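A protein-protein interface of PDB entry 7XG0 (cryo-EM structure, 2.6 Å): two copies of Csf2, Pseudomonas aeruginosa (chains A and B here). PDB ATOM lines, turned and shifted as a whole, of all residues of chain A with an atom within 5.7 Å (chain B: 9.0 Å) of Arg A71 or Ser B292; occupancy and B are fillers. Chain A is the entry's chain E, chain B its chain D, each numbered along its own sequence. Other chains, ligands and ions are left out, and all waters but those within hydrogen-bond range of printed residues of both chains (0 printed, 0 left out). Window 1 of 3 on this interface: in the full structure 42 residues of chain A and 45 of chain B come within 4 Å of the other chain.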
ATOM      1  N   PRO A  66      22.067  -5.996 -15.287  1.00  0.00           N
ATOM      2  CA  PRO A  66      21.066  -6.412 -16.283  1.00  0.00           C
ATOM      3  C   PRO A  66      19.641  -6.158 -15.812  1.00  0.00           C
ATOM      4  O   PRO A  66      19.354  -6.153 -14.614  1.00  0.00           O
ATOM      5  CB  PRO A  66      21.332  -7.912 -16.453  1.00  0.00           C
ATOM      6  CG  PRO A  66      22.698  -8.137 -15.941  1.00  0.00           C
ATOM      7  CD  PRO A  66      22.949  -7.107 -14.891  1.00  0.00           C
ATOM      8  N   GLY A  67      18.751  -5.926 -16.781  1.00  0.00           N
ATOM      9  CA  GLY A  67      17.354  -5.697 -16.458  1.00  0.00           C
ATOM     10  C   GLY A  67      16.661  -6.933 -15.925  1.00  0.00           C
ATOM     11  O   GLY A  67      15.653  -6.830 -15.226  1.00  0.00           O
ATOM     12  N   ASN A  68      17.189  -8.115 -16.252  1.00  0.00           N
ATOM     13  CA  ASN A  68      16.728  -9.349 -15.625  1.00  0.00           C
ATOM     14  C   ASN A  68      17.030  -9.358 -14.130  1.00  0.00           C
ATOM     15  O   ASN A  68      16.172  -9.728 -13.317  1.00  0.00           O
ATOM     16  CB  ASN A  68      17.391 -10.539 -16.313  1.00  0.00           C
ATOM     17  CG  ASN A  68      16.567 -11.796 -16.236  1.00  0.00           C
ATOM     18  OD1 ASN A  68      15.340 -11.753 -16.148  1.00  0.00           O
ATOM     19  ND2 ASN A  68      17.244 -12.936 -16.258  1.00  0.00           N
ATOM     20  N   THR A  69      18.241  -8.928 -13.755  1.00  0.00           N
ATOM     21  CA  THR A  69      18.644  -8.896 -12.349  1.00  0.00           C
ATOM     22  C   THR A  69      17.819  -7.885 -11.561  1.00  0.00           C
ATOM     23  O   THR A  69      17.316  -8.187 -10.473  1.00  0.00           O
ATOM     24  CB  THR A  69      20.136  -8.566 -12.248  1.00  0.00           C
ATOM     25  OG1 THR A  69      20.905  -9.622 -12.830  1.00  0.00           O
ATOM     26  CG2 THR A  69      20.559  -8.403 -10.800  1.00  0.00           C
ATOM     27  N   MET A  70      17.640  -6.686 -12.119  1.00  0.00           N
ATOM     28  CA  MET A  70      16.856  -5.660 -11.440  1.00  0.00           C
ATOM     29  C   MET A  70      15.369  -5.997 -11.426  1.00  0.00           C
ATOM     30  O   MET A  70      14.669  -5.648 -10.467  1.00  0.00           O
ATOM     31  CB  MET A  70      17.100  -4.304 -12.098  1.00  0.00           C
ATOM     32  CG  MET A  70      18.560  -3.907 -12.172  1.00  0.00           C
ATOM     33  SD  MET A  70      19.161  -3.313 -10.581  1.00  0.00           S
ATOM     34  CE  MET A  70      18.140  -1.861 -10.353  1.00  0.00           C
ATOM     35  N   ARG A  71      14.877  -6.679 -12.466  1.00  0.00           N
ATOM     36  CA  ARG A  71      13.494  -7.149 -12.471  1.00  0.00           C
ATOM     37  C   ARG A  71      13.261  -8.186 -11.384  1.00  0.00           C
ATOM     38  O   ARG A  71      12.249  -8.135 -10.677  1.00  0.00           O
ATOM     39  CB  ARG A  71      13.141  -7.732 -13.838  1.00  0.00           C
ATOM     40  CG  ARG A  71      11.710  -8.227 -13.938  1.00  0.00           C
ATOM     41  CD  ARG A  71      11.315  -8.498 -15.373  1.00  0.00           C
ATOM     42  NE  ARG A  71      10.006  -9.132 -15.461  1.00  0.00           N
ATOM     43  CZ  ARG A  71       8.882  -8.487 -15.737  1.00  0.00           C
ATOM     44  NH1 ARG A  71       8.869  -7.183 -15.951  1.00  0.00           N
ATOM     45  NH2 ARG A  71       7.744  -9.172 -15.813  1.00  0.00           N
ATOM     46  N   SER A  72      14.199  -9.124 -11.225  1.00  0.00           N
ATOM     47  CA  SER A  72      14.078 -10.099 -10.150  1.00  0.00           C
ATOM     48  C   SER A  72      14.253  -9.453  -8.783  1.00  0.00           C
ATOM     49  O   SER A  72      13.637  -9.902  -7.819  1.00  0.00           O
ATOM     50  CB  SER A  72      15.087 -11.224 -10.332  1.00  0.00           C
ATOM     51  OG  SER A  72      14.808 -12.301  -9.455  1.00  0.00           O
ATOM     52  N   LEU A  73      15.067  -8.398  -8.686  1.00  0.00           N
ATOM     53  CA  LEU A  73      15.200  -7.662  -7.429  1.00  0.00           C
ATOM     54  C   LEU A  73      13.890  -6.986  -7.039  1.00  0.00           C
ATOM     55  O   LEU A  73      13.457  -7.066  -5.881  1.00  0.00           O
ATOM     56  CB  LEU A  73      16.315  -6.624  -7.551  1.00  0.00           C
ATOM     57  CG  LEU A  73      16.417  -5.610  -6.410  1.00  0.00           C
ATOM     58  CD1 LEU A  73      16.804  -6.281  -5.098  1.00  0.00           C
ATOM     59  CD2 LEU A  73      17.382  -4.496  -6.764  1.00  0.00           C
ATOM     60  N   LEU A  74      13.246  -6.326  -8.006  1.00  0.00           N
ATOM     61  CA  LEU A  74      11.951  -5.687  -7.778  1.00  0.00           C
ATOM     62  C   LEU A  74      10.882  -6.717  -7.430  1.00  0.00           C
ATOM     63  O   LEU A  74      10.059  -6.506  -6.528  1.00  0.00           O
ATOM     64  CB  LEU A  74      11.561  -4.892  -9.023  1.00  0.00           C
ATOM     65  CG  LEU A  74      10.488  -3.812  -8.944  1.00  0.00           C
ATOM     66  CD1 LEU A  74      10.897  -2.677  -8.024  1.00  0.00           C
ATOM     67  CD2 LEU A  74      10.180  -3.293 -10.339  1.00  0.00           C
ATOM     68  N   ARG A  75      10.908  -7.859  -8.121  1.00  0.00           N
ATOM     69  CA  ARG A  75       9.976  -8.947  -7.846  1.00  0.00           C
ATOM     70  C   ARG A  75      10.191  -9.521  -6.450  1.00  0.00           C
ATOM     71  O   ARG A  75       9.228  -9.802  -5.728  1.00  0.00           O
ATOM     72  CB  ARG A  75      10.137 -10.032  -8.909  1.00  0.00           C
ATOM     73  CG  ARG A  75       9.267 -11.243  -8.711  1.00  0.00           C
ATOM     74  CD  ARG A  75       9.926 -12.462  -9.297  1.00  0.00           C
ATOM     75  NE  ARG A  75       9.901 -12.462 -10.755  1.00  0.00           N
ATOM     76  CZ  ARG A  75       8.915 -12.960 -11.488  1.00  0.00           C
ATOM     77  NH1 ARG A  75       7.850 -13.512 -10.930  1.00  0.00           N
ATOM     78  NH2 ARG A  75       8.999 -12.905 -12.814  1.00  0.00           N
ATOM     79  N   ARG A  76      11.453  -9.664  -6.038  1.00  0.00           N
ATOM     80  CA  ARG A  76      11.744 -10.266  -4.744  1.00  0.00           C
ATOM     81  C   ARG A  76      11.432  -9.315  -3.596  1.00  0.00           C
ATOM     82  O   ARG A  76      11.011  -9.766  -2.527  1.00  0.00           O
ATOM     83  CB  ARG A  76      13.198 -10.735  -4.692  1.00  0.00           C
ATOM     84  CG  ARG A  76      13.423 -12.052  -5.427  1.00  0.00           C
ATOM     85  CD  ARG A  76      14.876 -12.495  -5.453  1.00  0.00           C
ATOM     86  NE  ARG A  76      15.754 -11.549  -6.131  1.00  0.00           N
ATOM     87  CZ  ARG A  76      16.652 -10.791  -5.518  1.00  0.00           C
ATOM     88  NH1 ARG A  76      16.808 -10.829  -4.205  1.00  0.00           N
ATOM     89  NH2 ARG A  76      17.418  -9.980  -6.241  1.00  0.00           N
ATOM     90  N   LEU A 132       2.084  -7.664 -13.110  1.00  0.00           N
ATOM     91  CA  LEU A 132       3.444  -7.158 -13.280  1.00  0.00           C
ATOM     92  C   LEU A 132       4.365  -8.221 -13.874  1.00  0.00           C
ATOM     93  O   LEU A 132       5.180  -7.929 -14.755  1.00  0.00           O
ATOM     94  CB  LEU A 132       3.987  -6.644 -11.948  1.00  0.00           C
ATOM     95  CG  LEU A 132       3.341  -5.338 -11.477  1.00  0.00           C
ATOM     96  CD1 LEU A 132       3.871  -4.916 -10.122  1.00  0.00           C
ATOM     97  CD2 LEU A 132       3.514  -4.237 -12.500  1.00  0.00           C
ATOM     98  N   PHE A 133       4.240  -9.463 -13.422  1.00  0.00           N
ATOM     99  CA  PHE A 133       5.114 -10.540 -13.872  1.00  0.00           C
ATOM    100  C   PHE A 133       4.271 -11.683 -14.415  1.00  0.00           C
ATOM    101  O   PHE A 133       3.584 -12.372 -13.652  1.00  0.00           O
ATOM    102  CB  PHE A 133       6.024 -11.026 -12.743  1.00  0.00           C
ATOM    103  CG  PHE A 133       6.761  -9.920 -12.050  1.00  0.00           C
ATOM    104  CD1 PHE A 133       7.974  -9.468 -12.540  1.00  0.00           C
ATOM    105  CD2 PHE A 133       6.229  -9.317 -10.924  1.00  0.00           C
ATOM    106  CE1 PHE A 133       8.648  -8.441 -11.912  1.00  0.00           C
ATOM    107  CE2 PHE A 133       6.893  -8.295 -10.295  1.00  0.00           C
ATOM    108  CZ  PHE A 133       8.102  -7.850 -10.790  1.00  0.00           C
ATOM    109  N   GLY A 134       4.348 -11.897 -15.724  1.00  0.00           N
ATOM    110  CA  GLY A 134       3.600 -12.959 -16.358  1.00  0.00           C
ATOM    111  C   GLY A 134       4.296 -14.298 -16.252  1.00  0.00           C
ATOM    112  O   GLY A 134       4.718 -14.704 -15.165  1.00  0.00           O
ATOM    113  N   GLY A 142       3.647 -10.078 -18.777  1.00  0.00           N
ATOM    114  CA  GLY A 142       3.479  -9.083 -17.745  1.00  0.00           C
ATOM    115  C   GLY A 142       3.459  -7.670 -18.298  1.00  0.00           C
ATOM    116  O   GLY A 142       3.992  -7.396 -19.369  1.00  0.00           O
ATOM    117  N   LEU A 144       4.924  -5.176 -16.813  1.00  0.00           N
ATOM    118  CA  LEU A 144       6.108  -4.486 -16.319  1.00  0.00           C
ATOM    119  C   LEU A 144       7.262  -4.716 -17.286  1.00  0.00           C
ATOM    120  O   LEU A 144       7.427  -5.820 -17.816  1.00  0.00           O
ATOM    121  CB  LEU A 144       6.466  -4.963 -14.912  1.00  0.00           C
ATOM    122  CG  LEU A 144       7.503  -4.166 -14.129  1.00  0.00           C
ATOM    123  CD1 LEU A 144       6.852  -2.950 -13.535  1.00  0.00           C
ATOM    124  CD2 LEU A 144       8.066  -5.028 -13.027  1.00  0.00           C
ATOM    125  N   MET A 145       8.055  -3.672 -17.506  1.00  0.00           N
ATOM    126  CA  MET A 145       9.091  -3.637 -18.525  1.00  0.00           C
ATOM    127  C   MET A 145      10.341  -3.035 -17.895  1.00  0.00           C
ATOM    128  O   MET A 145      10.418  -1.818 -17.710  1.00  0.00           O
ATOM    129  CB  MET A 145       8.603  -2.810 -19.718  1.00  0.00           C
ATOM    130  CG  MET A 145       7.891  -3.634 -20.778  1.00  0.00           C
ATOM    131  SD  MET A 145       6.982  -2.754 -22.063  1.00  0.00           S
ATOM    132  CE  MET A 145       6.376  -1.331 -21.179  1.00  0.00           C
ATOM    133  N   VAL A 146      11.304  -3.880 -17.544  1.00  0.00           N
ATOM    134  CA  VAL A 146      12.392  -3.486 -16.656  1.00  0.00           C
ATOM    135  C   VAL A 146      13.672  -3.343 -17.467  1.00  0.00           C
ATOM    136  O   VAL A 146      14.223  -4.332 -17.963  1.00  0.00           O
ATOM    137  CB  VAL A 146      12.574  -4.486 -15.510  1.00  0.00           C
ATOM    138  CG1 VAL A 146      13.778  -4.118 -14.677  1.00  0.00           C
ATOM    139  CG2 VAL A 146      11.334  -4.514 -14.655  1.00  0.00           C
ATOM    140  N   ASP A 147      14.158  -2.110 -17.575  1.00  0.00           N
ATOM    141  CA  ASP A 147      15.405  -1.832 -18.267  1.00  0.00           C
ATOM    142  C   ASP A 147      16.591  -2.148 -17.358  1.00  0.00           C
ATOM    143  O   ASP A 147      16.450  -2.367 -16.150  1.00  0.00           O
ATOM    144  CB  ASP A 147      15.437  -0.375 -18.717  1.00  0.00           C
ATOM    145  CG  ASP A 147      16.309  -0.152 -19.927  1.00  0.00           C
ATOM    146  OD1 ASP A 147      16.833  -1.140 -20.483  1.00  0.00           O
ATOM    147  OD2 ASP A 147      16.470   1.023 -20.317  1.00  0.00           O
ATOM    148  N   TRP A 260      17.229   3.843 -13.633  1.00  0.00           N
ATOM    149  CA  TRP A 260      16.528   2.575 -13.790  1.00  0.00           C
ATOM    150  C   TRP A 260      15.177   2.842 -14.435  1.00  0.00           C
ATOM    151  O   TRP A 260      14.293   3.424 -13.802  1.00  0.00           O
ATOM    152  CB  TRP A 260      16.352   1.900 -12.432  1.00  0.00           C
ATOM    153  CG  TRP A 260      15.853   0.513 -12.510  1.00  0.00           C
ATOM    154  CD1 TRP A 260      15.965  -0.339 -13.564  1.00  0.00           C
ATOM    155  CD2 TRP A 260      15.163  -0.202 -11.483  1.00  0.00           C
ATOM    156  NE1 TRP A 260      15.383  -1.541 -13.261  1.00  0.00           N
ATOM    157  CE2 TRP A 260      14.882  -1.485 -11.988  1.00  0.00           C
ATOM    158  CE3 TRP A 260      14.755   0.118 -10.186  1.00  0.00           C
ATOM    159  CZ2 TRP A 260      14.206  -2.445 -11.243  1.00  0.00           C
ATOM    160  CZ3 TRP A 260      14.089  -0.838  -9.449  1.00  0.00           C
ATOM    161  CH2 TRP A 260      13.827  -2.105  -9.978  1.00  0.00           C
ATOM    162  N   PHE B  14      15.886  -6.734 -29.631  1.00  0.00           N
ATOM    163  CA  PHE B  14      15.897  -8.195 -29.628  1.00  0.00           C
ATOM    164  C   PHE B  14      14.728  -8.701 -30.467  1.00  0.00           C
ATOM    165  O   PHE B  14      13.612  -8.855 -29.962  1.00  0.00           O
ATOM    166  CB  PHE B  14      15.834  -8.740 -28.207  1.00  0.00           C
ATOM    167  CG  PHE B  14      15.878 -10.235 -28.134  1.00  0.00           C
ATOM    168  CD1 PHE B  14      16.881 -10.941 -28.777  1.00  0.00           C
ATOM    169  CD2 PHE B  14      14.920 -10.936 -27.417  1.00  0.00           C
ATOM    170  CE1 PHE B  14      16.927 -12.321 -28.714  1.00  0.00           C
ATOM    171  CE2 PHE B  14      14.960 -12.316 -27.348  1.00  0.00           C
ATOM    172  CZ  PHE B  14      15.967 -13.008 -27.996  1.00  0.00           C
ATOM    173  N   HIS B 249      21.107 -14.700 -25.098  1.00  0.00           N
ATOM    174  CA  HIS B 249      20.399 -14.173 -26.251  1.00  0.00           C
ATOM    175  C   HIS B 249      21.178 -12.991 -26.802  1.00  0.00           C
ATOM    176  O   HIS B 249      21.632 -12.129 -26.046  1.00  0.00           O
ATOM    177  CB  HIS B 249      18.956 -13.776 -25.897  1.00  0.00           C
ATOM    178  CG  HIS B 249      18.851 -12.798 -24.767  1.00  0.00           C
ATOM    179  ND1 HIS B 249      18.968 -13.172 -23.445  1.00  0.00           N
ATOM    180  CD2 HIS B 249      18.618 -11.465 -24.760  1.00  0.00           C
ATOM    181  CE1 HIS B 249      18.824 -12.110 -22.674  1.00  0.00           C
ATOM    182  NE2 HIS B 249      18.611 -11.060 -23.447  1.00  0.00           N
ATOM    183  N   ARG B 286       7.118  -0.847 -28.002  1.00  0.00           N
ATOM    184  CA  ARG B 286       8.296  -1.700 -28.085  1.00  0.00           C
ATOM    185  C   ARG B 286       8.398  -2.267 -29.493  1.00  0.00           C
ATOM    186  O   ARG B 286       7.397  -2.727 -30.053  1.00  0.00           O
ATOM    187  CB  ARG B 286       8.229  -2.825 -27.049  1.00  0.00           C
ATOM    188  CG  ARG B 286       8.286  -2.336 -25.605  1.00  0.00           C
ATOM    189  CD  ARG B 286       9.398  -1.318 -25.398  1.00  0.00           C
ATOM    190  NE  ARG B 286       9.278  -0.618 -24.125  1.00  0.00           N
ATOM    191  CZ  ARG B 286       8.801   0.613 -23.993  1.00  0.00           C
ATOM    192  NH1 ARG B 286       8.390   1.311 -25.039  1.00  0.00           N
ATOM    193  NH2 ARG B 286       8.737   1.157 -22.781  1.00  0.00           N
ATOM    194  N   GLY B 289      10.708  -7.280 -29.423  1.00  0.00           N
ATOM    195  CA  GLY B 289      10.496  -8.386 -28.513  1.00  0.00           C
ATOM    196  C   GLY B 289      11.407  -8.269 -27.315  1.00  0.00           C
ATOM    197  O   GLY B 289      12.157  -7.302 -27.178  1.00  0.00           O
ATOM    198  N   GLY B 290      11.349  -9.285 -26.458  1.00  0.00           N
ATOM    199  CA  GLY B 290      11.986  -9.211 -25.159  1.00  0.00           C
ATOM    200  C   GLY B 290      11.285  -8.187 -24.294  1.00  0.00           C
ATOM    201  O   GLY B 290      11.877  -7.163 -23.937  1.00  0.00           O
ATOM    202  N   HIS B 291      10.014  -8.453 -23.970  1.00  0.00           N
ATOM    203  CA  HIS B 291       9.169  -7.449 -23.327  1.00  0.00           C
ATOM    204  C   HIS B 291       9.644  -7.151 -21.912  1.00  0.00           C
ATOM    205  O   HIS B 291       9.876  -5.992 -21.560  1.00  0.00           O
ATOM    206  CB  HIS B 291       7.716  -7.922 -23.306  1.00  0.00           C
ATOM    207  CG  HIS B 291       6.734  -6.853 -22.945  1.00  0.00           C
ATOM    208  ND1 HIS B 291       6.029  -6.853 -21.761  1.00  0.00           N
ATOM    209  CD2 HIS B 291       6.332  -5.753 -23.623  1.00  0.00           C
ATOM    210  CE1 HIS B 291       5.238  -5.795 -21.722  1.00  0.00           C
ATOM    211  NE2 HIS B 291       5.406  -5.110 -22.839  1.00  0.00           N
ATOM    212  N   SER B 292       9.865  -8.197 -21.112  1.00  0.00           N
ATOM    213  CA  SER B 292      10.089  -8.008 -19.683  1.00  0.00           C
ATOM    214  C   SER B 292      11.460  -7.410 -19.383  1.00  0.00           C
ATOM    215  O   SER B 292      11.680  -6.893 -18.280  1.00  0.00           O
ATOM    216  CB  SER B 292       9.914  -9.336 -18.957  1.00  0.00           C
ATOM    217  OG  SER B 292      10.695 -10.359 -19.548  1.00  0.00           O
ATOM    218  N   LYS B 293      12.384  -7.452 -20.340  1.00  0.00           N
ATOM    219  CA  LYS B 293      13.668  -6.778 -20.211  1.00  0.00           C
ATOM    220  C   LYS B 293      13.647  -5.376 -20.812  1.00  0.00           C
ATOM    221  O   LYS B 293      14.715  -4.788 -21.024  1.00  0.00           O
ATOM    222  CB  LYS B 293      14.774  -7.623 -20.845  1.00  0.00           C
ATOM    223  CG  LYS B 293      14.520  -9.117 -20.749  1.00  0.00           C
ATOM    224  CD  LYS B 293      15.705  -9.925 -21.239  1.00  0.00           C
ATOM    225  CE  LYS B 293      15.442 -11.411 -21.085  1.00  0.00           C
ATOM    226  NZ  LYS B 293      16.484 -12.072 -20.256  1.00  0.00           N
ATOM    227  N   ASP B 294      12.449  -4.844 -21.091  1.00  0.00           N
ATOM    228  CA  ASP B 294      12.196  -3.511 -21.651  1.00  0.00           C
ATOM    229  C   ASP B 294      12.873  -3.296 -23.000  1.00  0.00           C
ATOM    230  O   ASP B 294      13.159  -2.155 -23.375  1.00  0.00           O
ATOM    231  CB  ASP B 294      12.602  -2.390 -20.685  1.00  0.00           C
ATOM    232  CG  ASP B 294      11.680  -1.186 -20.764  1.00  0.00           C
ATOM    233  OD1 ASP B 294      10.935  -1.069 -21.759  1.00  0.00           O
ATOM    234  OD2 ASP B 294      11.716  -0.344 -19.842  1.00  0.00           O
ATOM    235  N   TYR B 295      13.127  -4.368 -23.744  1.00  0.00           N
ATOM    236  CA  TYR B 295      13.791  -4.241 -25.030  1.00  0.00           C
ATOM    237  C   TYR B 295      12.822  -3.680 -26.065  1.00  0.00           C
ATOM    238  O   TYR B 295      11.604  -3.847 -25.964  1.00  0.00           O
ATOM    239  CB  TYR B 295      14.329  -5.598 -25.490  1.00  0.00           C
ATOM    240  CG  TYR B 295      15.498  -6.144 -24.694  1.00  0.00           C
ATOM    241  CD1 TYR B 295      16.239  -5.328 -23.845  1.00  0.00           C
ATOM    242  CD2 TYR B 295      15.858  -7.483 -24.795  1.00  0.00           C
ATOM    243  CE1 TYR B 295      17.304  -5.834 -23.118  1.00  0.00           C
ATOM    244  CE2 TYR B 295      16.922  -7.996 -24.075  1.00  0.00           C
ATOM    245  CZ  TYR B 295      17.640  -7.166 -23.238  1.00  0.00           C
ATOM    246  OH  TYR B 295      18.698  -7.675 -22.521  1.00  0.00           O
ATOM    247  N   GLY B 296      13.375  -3.000 -27.068  1.00  0.00           N
ATOM    248  CA  GLY B 296      12.592  -2.434 -28.144  1.00  0.00           C
ATOM    249  C   GLY B 296      12.139  -1.003 -27.937  1.00  0.00           C
ATOM    250  O   GLY B 296      11.509  -0.439 -28.840  1.00  0.00           O
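No position is printed for both chains.
Of the 10 pairs that touch across the chains among the printed residues, none has its exchanged pair printed and touching as well.
Among the printed residues, pairs that only touch across the chains: Arg A71 with Ser B292 (3.3 Å), Asp A147 with Asp B294 (3.5 Å), Val A146 with Asp B294 (3.5 Å) and Leu A144 with Ser B292 (3.9 Å).
The side-chain sulfur (SD) of Met A145 lies within hydrogen-bond range of the guanidinium group (NE) of Arg B286 (3.8 Å).
O of Gly A142 lies close to ND1 of His B291, at 3.2 Å.
NE2 of His B291 sits at hydrogen-bond distance from SD of Met A145 (2.9 Å).
The backbone carbonyl oxygen (O) of Ser B292 sits at hydrogen-bond distance from the backbone NH (N) of Val A146 (3.1 Å).
The side-chain carboxylate of Asp B294 lies close to the backbone carbonyl oxygen of Met A145 (2.9 Å).
The backbone carbonyl oxygen (O) of Val A146 sits close to the backbone carbonyl oxygen (O) of Lys B293 (3.1 Å).
Of the 11 printed residues of chain B, 5 touch a printed residue of chain A.
Hydrophobic or aromatic side chains of chain B within 4 Å of the printed part of chain A: His B291.
Among the printed residues, 10 pairs touch across the chains.
Among the printed residues, no Asp or Glu carboxylate lies within 4 Å of a Lys or Arg side-chain nitrogen of the other chain.
OD1 of Asp B294 is in salt-bridge range of NE of Arg B286 (2.9 Å).
O of Leu A132 sits at hydrogen-bond distance from NH2 of Arg A71 (3.0 Å).
O of Leu A144 is in hydrogen-bond range of NH1 of Arg A71 (2.7 Å).
The backbone carbonyl oxygen (O) of Leu A132 sits close to the backbone NH (N) of Leu A144 (3.4 Å).
O of Asp A147 lies within hydrogen-bond range of NE1 of Trp A260 (3.2 Å).
Of chain A, only Arg A71, Leu A144 and Val A146 come within 4 Å of Ser B292.
No residue of chain B comes within 4 Å of Ser A72.
Printed residues of chain B within 4 Å of Val A146: Ser B292 (3.1 Å), Lys B293 (3.1 Å) and Asp B294 (3.5 Å).
Printed residues of chain A within 4 Å of Asp B294: Met A145 (2.9 Å), Val A146 (3.5 Å) and Asp A147 (3.5 Å).
Of the printed residues of chain A, Lys B293 touches Val A146.
Pro A66 touches none of the printed residues of chain B.
The nearest residue of chain A that does not touch Ser B292 is Met A145 (4.1 Å).
The nearest printed residue of chain B that does not touch Met A145 is Ser B292 (4.1 Å).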
